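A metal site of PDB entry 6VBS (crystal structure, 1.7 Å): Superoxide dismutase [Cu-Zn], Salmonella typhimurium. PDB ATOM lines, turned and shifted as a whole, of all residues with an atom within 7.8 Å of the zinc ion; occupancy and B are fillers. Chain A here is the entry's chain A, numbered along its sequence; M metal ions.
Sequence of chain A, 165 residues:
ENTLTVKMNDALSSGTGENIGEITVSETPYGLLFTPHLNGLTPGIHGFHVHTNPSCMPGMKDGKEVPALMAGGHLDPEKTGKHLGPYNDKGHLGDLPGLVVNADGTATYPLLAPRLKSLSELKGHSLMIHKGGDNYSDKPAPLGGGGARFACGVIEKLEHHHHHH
The side-chain carboxylate (OD2) of Asp 95 is in hydrogen-bond range of the backbone NH (N) of Leu 84 (3.2 Å). OD2 of Asp 95 sits at hydrogen-bond distance from N of Gly 85, at 3.1 Å. NE2 of His 83 sits at hydrogen-bond distance from OD1 of Asp 134 (2.8 Å). The backbone NH (N) of His 83 lies within hydrogen-bond range of the side-chain carboxylate (OD2) of Asp 138 (2.8 Å). N of His 92 is in hydrogen-bond range of O of Lys 82 (2.8 Å). N of His 92 sits at hydrogen-bond distance from OG1 of Thr 80 (3.3 Å). The backbone carbonyl oxygen (O) of His 92 lies within hydrogen-bond range of the guanidinium group (NH1) of Arg 115 (3.0 Å). A ring nitrogen (ND1) of His 49 lies close to a ring nitrogen (NE2) of His 74.
Along chain A the residues within 4 Å of the zinc ion span positions 74 to 95. The nearest printed residue that does not touch the zinc ion is Leu 143 (4.7 Å).
The zinc ion is bound by OD1 of Asp 95 (1.9 Å), ND1 of His 83 (2.0 Å), ND1 of His 92 (2.0 Å) and ND1 of His 74 (2.0 Å). The zinc ion has four donor atoms within binding distance.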
ATOM      1  N   PHE A  48       6.299  -3.095  11.773  1.00  0.00           N
ATOM      2  CA  PHE A  48       7.690  -2.798  11.474  1.00  0.00           C
ATOM      3  C   PHE A  48       7.906  -1.332  11.787  1.00  0.00           C
ATOM      4  O   PHE A  48       7.323  -0.472  11.124  1.00  0.00           O
ATOM      5  CB  PHE A  48       7.966  -3.118  10.007  1.00  0.00           C
ATOM      6  CG  PHE A  48       9.363  -2.889   9.541  1.00  0.00           C
ATOM      7  CD1 PHE A  48      10.453  -3.318  10.279  1.00  0.00           C
ATOM      8  CD2 PHE A  48       9.584  -2.294   8.321  1.00  0.00           C
ATOM      9  CE1 PHE A  48      11.735  -3.122   9.803  1.00  0.00           C
ATOM     10  CE2 PHE A  48      10.860  -2.102   7.838  1.00  0.00           C
ATOM     11  CZ  PHE A  48      11.929  -2.501   8.577  1.00  0.00           C
ATOM     12  N   HIS A  49       8.716  -1.051  12.815  1.00  0.00           N
ATOM     13  CA  HIS A  49       8.913   0.309  13.294  1.00  0.00           C
ATOM     14  C   HIS A  49      10.356   0.568  13.717  1.00  0.00           C
ATOM     15  O   HIS A  49      11.102  -0.347  14.086  1.00  0.00           O
ATOM     16  CB  HIS A  49       7.992   0.613  14.471  1.00  0.00           C
ATOM     17  CG  HIS A  49       6.678  -0.097  14.416  1.00  0.00           C
ATOM     18  ND1 HIS A  49       6.338  -1.133  15.260  1.00  0.00           N
ATOM     19  CD2 HIS A  49       5.588   0.126  13.643  1.00  0.00           C
ATOM     20  CE1 HIS A  49       5.101  -1.533  14.982  1.00  0.00           C
ATOM     21  NE2 HIS A  49       4.622  -0.783  14.014  1.00  0.00           N
ATOM     22  N   VAL A  50      10.742   1.841  13.614  1.00  0.00           N
ATOM     23  CA  VAL A  50      11.945   2.346  14.268  1.00  0.00           C
ATOM     24  C   VAL A  50      11.600   2.660  15.722  1.00  0.00           C
ATOM     25  O   VAL A  50      10.653   3.399  16.013  1.00  0.00           O
ATOM     26  CB  VAL A  50      12.479   3.599  13.553  1.00  0.00           C
ATOM     27  CG1 VAL A  50      13.837   3.963  14.129  1.00  0.00           C
ATOM     28  CG2 VAL A  50      12.565   3.374  12.080  1.00  0.00           C
ATOM     29  N   HIS A  51      12.350   2.085  16.631  1.00  0.00           N
ATOM     30  CA  HIS A  51      12.218   2.358  18.048  1.00  0.00           C
ATOM     31  C   HIS A  51      13.346   3.276  18.510  1.00  0.00           C
ATOM     32  O   HIS A  51      14.407   3.384  17.890  1.00  0.00           O
ATOM     33  CB  HIS A  51      12.189   1.055  18.843  1.00  0.00           C
ATOM     34  CG  HIS A  51      10.903   0.284  18.693  1.00  0.00           C
ATOM     35  ND1 HIS A  51      10.114  -0.058  19.769  1.00  0.00           N
ATOM     36  CD2 HIS A  51      10.278  -0.223  17.605  1.00  0.00           C
ATOM     37  CE1 HIS A  51       9.065  -0.734  19.349  1.00  0.00           C
ATOM     38  NE2 HIS A  51       9.132  -0.831  18.036  1.00  0.00           N
ATOM     39  N   GLY A  73      10.060   2.741  22.996  1.00  0.00           N
ATOM     40  CA  GLY A  73       8.864   2.846  22.182  1.00  0.00           C
ATOM     41  C   GLY A  73       9.146   3.284  20.760  1.00  0.00           C
ATOM     42  O   GLY A  73      10.282   3.389  20.309  1.00  0.00           O
ATOM     43  N   HIS A  74       8.052   3.497  20.020  1.00  0.00           N
ATOM     44  CA  HIS A  74       8.189   3.959  18.647  1.00  0.00           C
ATOM     45  C   HIS A  74       8.870   5.329  18.621  1.00  0.00           C
ATOM     46  O   HIS A  74       8.543   6.201  19.425  1.00  0.00           O
ATOM     47  CB  HIS A  74       6.827   4.052  17.966  1.00  0.00           C
ATOM     48  CG  HIS A  74       6.150   2.726  17.812  1.00  0.00           C
ATOM     49  ND1 HIS A  74       4.995   2.563  17.069  1.00  0.00           N
ATOM     50  CD2 HIS A  74       6.462   1.501  18.299  1.00  0.00           C
ATOM     51  CE1 HIS A  74       4.636   1.292  17.102  1.00  0.00           C
ATOM     52  NE2 HIS A  74       5.505   0.628  17.855  1.00  0.00           N
ATOM     53  N   LEU A  75       9.819   5.490  17.714  1.00  0.00           N
ATOM     54  CA  LEU A  75      10.507   6.779  17.578  1.00  0.00           C
ATOM     55  C   LEU A  75       9.492   7.898  17.363  1.00  0.00           C
ATOM     56  O   LEU A  75       8.696   7.844  16.427  1.00  0.00           O
ATOM     57  CB  LEU A  75      11.498   6.701  16.430  1.00  0.00           C
ATOM     58  CG  LEU A  75      12.257   7.956  16.040  1.00  0.00           C
ATOM     59  CD1 LEU A  75      13.141   8.331  17.208  1.00  0.00           C
ATOM     60  CD2 LEU A  75      13.048   7.746  14.765  1.00  0.00           C
ATOM     61  N   ASP A  76       9.537   8.923  18.245  1.00  0.00           N
ATOM     62  CA  ASP A  76       8.491   9.950  18.301  1.00  0.00           C
ATOM     63  C   ASP A  76       9.061  11.277  18.786  1.00  0.00           C
ATOM     64  O   ASP A  76       8.627  11.811  19.808  1.00  0.00           O
ATOM     65  CB  ASP A  76       7.349   9.492  19.218  1.00  0.00           C
ATOM     66  CG  ASP A  76       6.106  10.366  19.117  1.00  0.00           C
ATOM     67  OD1 ASP A  76       5.888  11.075  18.092  1.00  0.00           O
ATOM     68  OD2 ASP A  76       5.297  10.293  20.082  1.00  0.00           O
ATOM     69  N   THR A  80       4.069  13.151  19.333  1.00  0.00           N
ATOM     70  CA  THR A  80       2.689  13.007  18.904  1.00  0.00           C
ATOM     71  C   THR A  80       1.892  12.110  19.841  1.00  0.00           C
ATOM     72  O   THR A  80       0.680  12.314  20.017  1.00  0.00           O
ATOM     73  CB  THR A  80       2.593  12.447  17.477  1.00  0.00           C
ATOM     74  OG1 THR A  80       3.089  11.092  17.418  1.00  0.00           O
ATOM     75  CG2 THR A  80       3.358  13.291  16.496  1.00  0.00           C
ATOM     76  N   GLY A  81       2.534  11.086  20.410  1.00  0.00           N
ATOM     77  CA  GLY A  81       1.816  10.108  21.201  1.00  0.00           C
ATOM     78  C   GLY A  81       0.811   9.288  20.440  1.00  0.00           C
ATOM     79  O   GLY A  81      -0.061   8.671  21.052  1.00  0.00           O
ATOM     80  N   LYS A  82       0.898   9.244  19.116  1.00  0.00           N
ATOM     81  CA  LYS A  82      -0.093   8.574  18.289  1.00  0.00           C
ATOM     82  C   LYS A  82       0.571   7.676  17.252  1.00  0.00           C
ATOM     83  O   LYS A  82       1.516   8.104  16.588  1.00  0.00           O
ATOM     84  CB  LYS A  82      -0.989   9.573  17.554  1.00  0.00           C
ATOM     85  CG  LYS A  82      -1.788  10.530  18.396  1.00  0.00           C
ATOM     86  CD  LYS A  82      -2.787  11.260  17.494  1.00  0.00           C
ATOM     87  CE  LYS A  82      -3.160  12.661  17.994  1.00  0.00           C
ATOM     88  NZ  LYS A  82      -3.735  12.651  19.366  1.00  0.00           N
ATOM     89  N   HIS A  83       0.027   6.470  17.069  1.00  0.00           N
ATOM     90  CA  HIS A  83       0.498   5.536  16.052  1.00  0.00           C
ATOM     91  C   HIS A  83      -0.431   5.654  14.842  1.00  0.00           C
ATOM     92  O   HIS A  83      -1.584   5.224  14.896  1.00  0.00           O
ATOM     93  CB  HIS A  83       0.534   4.106  16.576  1.00  0.00           C
ATOM     94  CG  HIS A  83       1.036   3.119  15.575  1.00  0.00           C
ATOM     95  ND1 HIS A  83       2.386   2.965  15.294  1.00  0.00           N
ATOM     96  CD2 HIS A  83       0.385   2.262  14.758  1.00  0.00           C
ATOM     97  CE1 HIS A  83       2.525   2.046  14.354  1.00  0.00           C
ATOM     98  NE2 HIS A  83       1.322   1.615  14.002  1.00  0.00           N
ATOM     99  N   LEU A  84       0.078   6.245  13.751  1.00  0.00           N
ATOM    100  CA  LEU A  84      -0.743   6.486  12.565  1.00  0.00           C
ATOM    101  C   LEU A  84      -0.101   6.054  11.249  1.00  0.00           C
ATOM    102  O   LEU A  84      -0.651   6.348  10.178  1.00  0.00           O
ATOM    103  CB  LEU A  84      -1.136   7.963  12.497  1.00  0.00           C
ATOM    104  CG  LEU A  84      -2.116   8.413  13.569  1.00  0.00           C
ATOM    105  CD1 LEU A  84      -2.177   9.924  13.713  1.00  0.00           C
ATOM    106  CD2 LEU A  84      -3.517   7.861  13.240  1.00  0.00           C
ATOM    107  N   GLY A  85       1.000   5.306  11.285  1.00  0.00           N
ATOM    108  CA  GLY A  85       1.553   4.714  10.104  1.00  0.00           C
ATOM    109  C   GLY A  85       2.517   5.600   9.331  1.00  0.00           C
ATOM    110  O   GLY A  85       2.802   6.750   9.690  1.00  0.00           O
ATOM    111  N   GLY A  91       1.471  11.159  13.458  1.00  0.00           N
ATOM    112  CA  GLY A  91       1.907  10.132  14.390  1.00  0.00           C
ATOM    113  C   GLY A  91       3.406   9.892  14.436  1.00  0.00           C
ATOM    114  O   GLY A  91       4.193  10.654  13.880  1.00  0.00           O
ATOM    115  N   HIS A  92       3.798   8.798  15.105  1.00  0.00           N
ATOM    116  CA  HIS A  92       5.210   8.496  15.317  1.00  0.00           C
ATOM    117  C   HIS A  92       6.009   8.560  14.026  1.00  0.00           C
ATOM    118  O   HIS A  92       5.674   7.898  13.032  1.00  0.00           O
ATOM    119  CB  HIS A  92       5.396   7.085  15.886  1.00  0.00           C
ATOM    120  CG  HIS A  92       4.553   6.764  17.079  1.00  0.00           C
ATOM    121  ND1 HIS A  92       3.916   5.546  17.213  1.00  0.00           N
ATOM    122  CD2 HIS A  92       4.307   7.463  18.208  1.00  0.00           C
ATOM    123  CE1 HIS A  92       3.273   5.535  18.371  1.00  0.00           C
ATOM    124  NE2 HIS A  92       3.504   6.673  18.995  1.00  0.00           N
ATOM    125  N   LEU A  93       7.117   9.292  14.057  1.00  0.00           N
ATOM    126  CA  LEU A  93       8.024   9.320  12.916  1.00  0.00           C
ATOM    127  C   LEU A  93       8.573   7.924  12.593  1.00  0.00           C
ATOM    128  O   LEU A  93       8.825   7.627  11.416  1.00  0.00           O
ATOM    129  CB  LEU A  93       9.167  10.290  13.214  1.00  0.00           C
ATOM    130  CG  LEU A  93      10.165  10.472  12.069  1.00  0.00           C
ATOM    131  CD1 LEU A  93       9.407  11.031  10.875  1.00  0.00           C
ATOM    132  CD2 LEU A  93      11.236  11.400  12.553  1.00  0.00           C
ATOM    133  N   GLY A  94       8.725   7.060  13.605  1.00  0.00           N
ATOM    134  CA  GLY A  94       9.268   5.736  13.394  1.00  0.00           C
ATOM    135  C   GLY A  94       8.354   4.715  12.756  1.00  0.00           C
ATOM    136  O   GLY A  94       8.746   3.560  12.609  1.00  0.00           O
ATOM    137  N   ASP A  95       7.129   5.091  12.420  1.00  0.00           N
ATOM    138  CA  ASP A  95       6.178   4.138  11.866  1.00  0.00           C
ATOM    139  C   ASP A  95       6.503   3.858  10.398  1.00  0.00           C
ATOM    140  O   ASP A  95       6.383   4.745   9.561  1.00  0.00           O
ATOM    141  CB  ASP A  95       4.757   4.677  11.965  1.00  0.00           C
ATOM    142  CG  ASP A  95       4.254   4.739  13.384  1.00  0.00           C
ATOM    143  OD1 ASP A  95       4.921   4.201  14.346  1.00  0.00           O
ATOM    144  OD2 ASP A  95       3.176   5.376  13.540  1.00  0.00           O
ATOM    145  N   LEU A  96       6.878   2.626  10.104  1.00  0.00           N
ATOM    146  CA  LEU A  96       7.210   2.181   8.772  1.00  0.00           C
ATOM    147  C   LEU A  96       6.074   1.350   8.197  1.00  0.00           C
ATOM    148  O   LEU A  96       5.194   0.881   8.927  1.00  0.00           O
ATOM    149  CB  LEU A  96       8.489   1.356   8.813  1.00  0.00           C
ATOM    150  CG  LEU A  96       9.647   1.986   9.570  1.00  0.00           C
ATOM    151  CD1 LEU A  96      10.762   0.991   9.724  1.00  0.00           C
ATOM    152  CD2 LEU A  96      10.119   3.259   8.849  1.00  0.00           C
ATOM    153  N   ARG A 115       8.301   9.438   4.882  1.00  0.00           N
ATOM    154  CA  ARG A 115       8.489  10.503   5.868  1.00  0.00           C
ATOM    155  C   ARG A 115       9.932  10.588   6.346  1.00  0.00           C
ATOM    156  O   ARG A 115      10.292  11.571   7.018  1.00  0.00           O
ATOM    157  CB  ARG A 115       7.565  10.284   7.057  1.00  0.00           C
ATOM    158  CG  ARG A 115       6.123  10.452   6.720  1.00  0.00           C
ATOM    159  CD  ARG A 115       5.221   9.973   7.859  1.00  0.00           C
ATOM    160  NE  ARG A 115       5.472  10.713   9.082  1.00  0.00           N
ATOM    161  CZ  ARG A 115       5.208  10.266  10.315  1.00  0.00           C
ATOM    162  NH1 ARG A 115       4.690   9.048  10.483  1.00  0.00           N
ATOM    163  NH2 ARG A 115       5.478  11.013  11.366  1.00  0.00           N
ATOM    164  N   ASP A 134      -0.050  -4.461  11.407  1.00  0.00           N
ATOM    165  CA  ASP A 134      -0.085  -3.010  11.613  1.00  0.00           C
ATOM    166  C   ASP A 134      -1.169  -2.399  10.720  1.00  0.00           C
ATOM    167  O   ASP A 134      -1.005  -2.338   9.503  1.00  0.00           O
ATOM    168  CB  ASP A 134       1.271  -2.363  11.318  1.00  0.00           C
ATOM    169  CG  ASP A 134       1.393  -0.969  11.897  1.00  0.00           C
ATOM    170  OD1 ASP A 134       0.369  -0.410  12.325  1.00  0.00           O
ATOM    171  OD2 ASP A 134       2.523  -0.429  11.924  1.00  0.00           O
ATOM    172  N   TYR A 136      -1.986   0.698  11.125  1.00  0.00           N
ATOM    173  CA  TYR A 136      -1.628   2.126  11.111  1.00  0.00           C
ATOM    174  C   TYR A 136      -2.552   2.949  11.996  1.00  0.00           C
ATOM    175  O   TYR A 136      -2.814   4.128  11.718  1.00  0.00           O
ATOM    176  CB  TYR A 136      -1.608   2.657   9.682  1.00  0.00           C
ATOM    177  CG  TYR A 136      -0.707   1.875   8.740  1.00  0.00           C
ATOM    178  CD1 TYR A 136       0.360   1.115   9.220  1.00  0.00           C
ATOM    179  CD2 TYR A 136      -0.911   1.894   7.366  1.00  0.00           C
ATOM    180  CE1 TYR A 136       1.180   0.404   8.366  1.00  0.00           C
ATOM    181  CE2 TYR A 136      -0.094   1.175   6.491  1.00  0.00           C
ATOM    182  CZ  TYR A 136       0.947   0.412   7.003  1.00  0.00           C
ATOM    183  OH  TYR A 136       1.755  -0.326   6.171  1.00  0.00           O
ATOM    184  N   SER A 137      -3.020   2.367  13.094  1.00  0.00           N
ATOM    185  CA  SER A 137      -3.929   3.048  13.996  1.00  0.00           C
ATOM    186  C   SER A 137      -3.709   2.540  15.406  1.00  0.00           C
ATOM    187  O   SER A 137      -3.093   1.496  15.626  1.00  0.00           O
ATOM    188  CB  SER A 137      -5.395   2.842  13.551  1.00  0.00           C
ATOM    189  OG  SER A 137      -6.314   3.443  14.446  1.00  0.00           O
ATOM    190  N   ASP A 138      -4.175   3.328  16.372  1.00  0.00           N
ATOM    191  CA  ASP A 138      -4.236   2.906  17.765  1.00  0.00           C
ATOM    192  C   ASP A 138      -5.559   2.213  18.097  1.00  0.00           C
ATOM    193  O   ASP A 138      -5.766   1.841  19.243  1.00  0.00           O
ATOM    194  CB  ASP A 138      -4.008   4.110  18.671  1.00  0.00           C
ATOM    195  CG  ASP A 138      -2.527   4.471  18.814  1.00  0.00           C
ATOM    196  OD1 ASP A 138      -1.703   3.572  19.135  1.00  0.00           O
ATOM    197  OD2 ASP A 138      -2.189   5.650  18.592  1.00  0.00           O
ATOM    198  N   LEU A 143      -0.921   0.637  18.991  1.00  0.00           N
ATOM    199  CA  LEU A 143       0.311   0.467  18.201  1.00  0.00           C
ATOM    200  C   LEU A 143       0.074  -0.461  17.017  1.00  0.00           C
ATOM    201  O   LEU A 143       0.932  -1.259  16.632  1.00  0.00           O
ATOM    202  CB  LEU A 143       1.454  -0.042  19.083  1.00  0.00           C
ATOM    203  CG  LEU A 143       1.672   0.836  20.317  1.00  0.00           C
ATOM    204  CD1 LEU A 143       2.767   0.307  21.255  1.00  0.00           C
ATOM    205  CD2 LEU A 143       1.981   2.299  19.970  1.00  0.00           C
ATOM    206  N   GLY A 144      -1.102  -0.342  16.416  1.00  0.00           N
ATOM    207  CA  GLY A 144      -1.421  -1.025  15.174  1.00  0.00           C
ATOM    208  C   GLY A 144      -1.715  -2.497  15.307  1.00  0.00           C
ATOM    209  O   GLY A 144      -1.913  -3.158  14.283  1.00  0.00           O
HETATM  210 ZN    ZN M   1       3.957   3.948  16.006  1.00  0.00          ZN
HETATM  211 CU    CU M   2       7.489  -1.509  16.945  1.00  0.00          CU
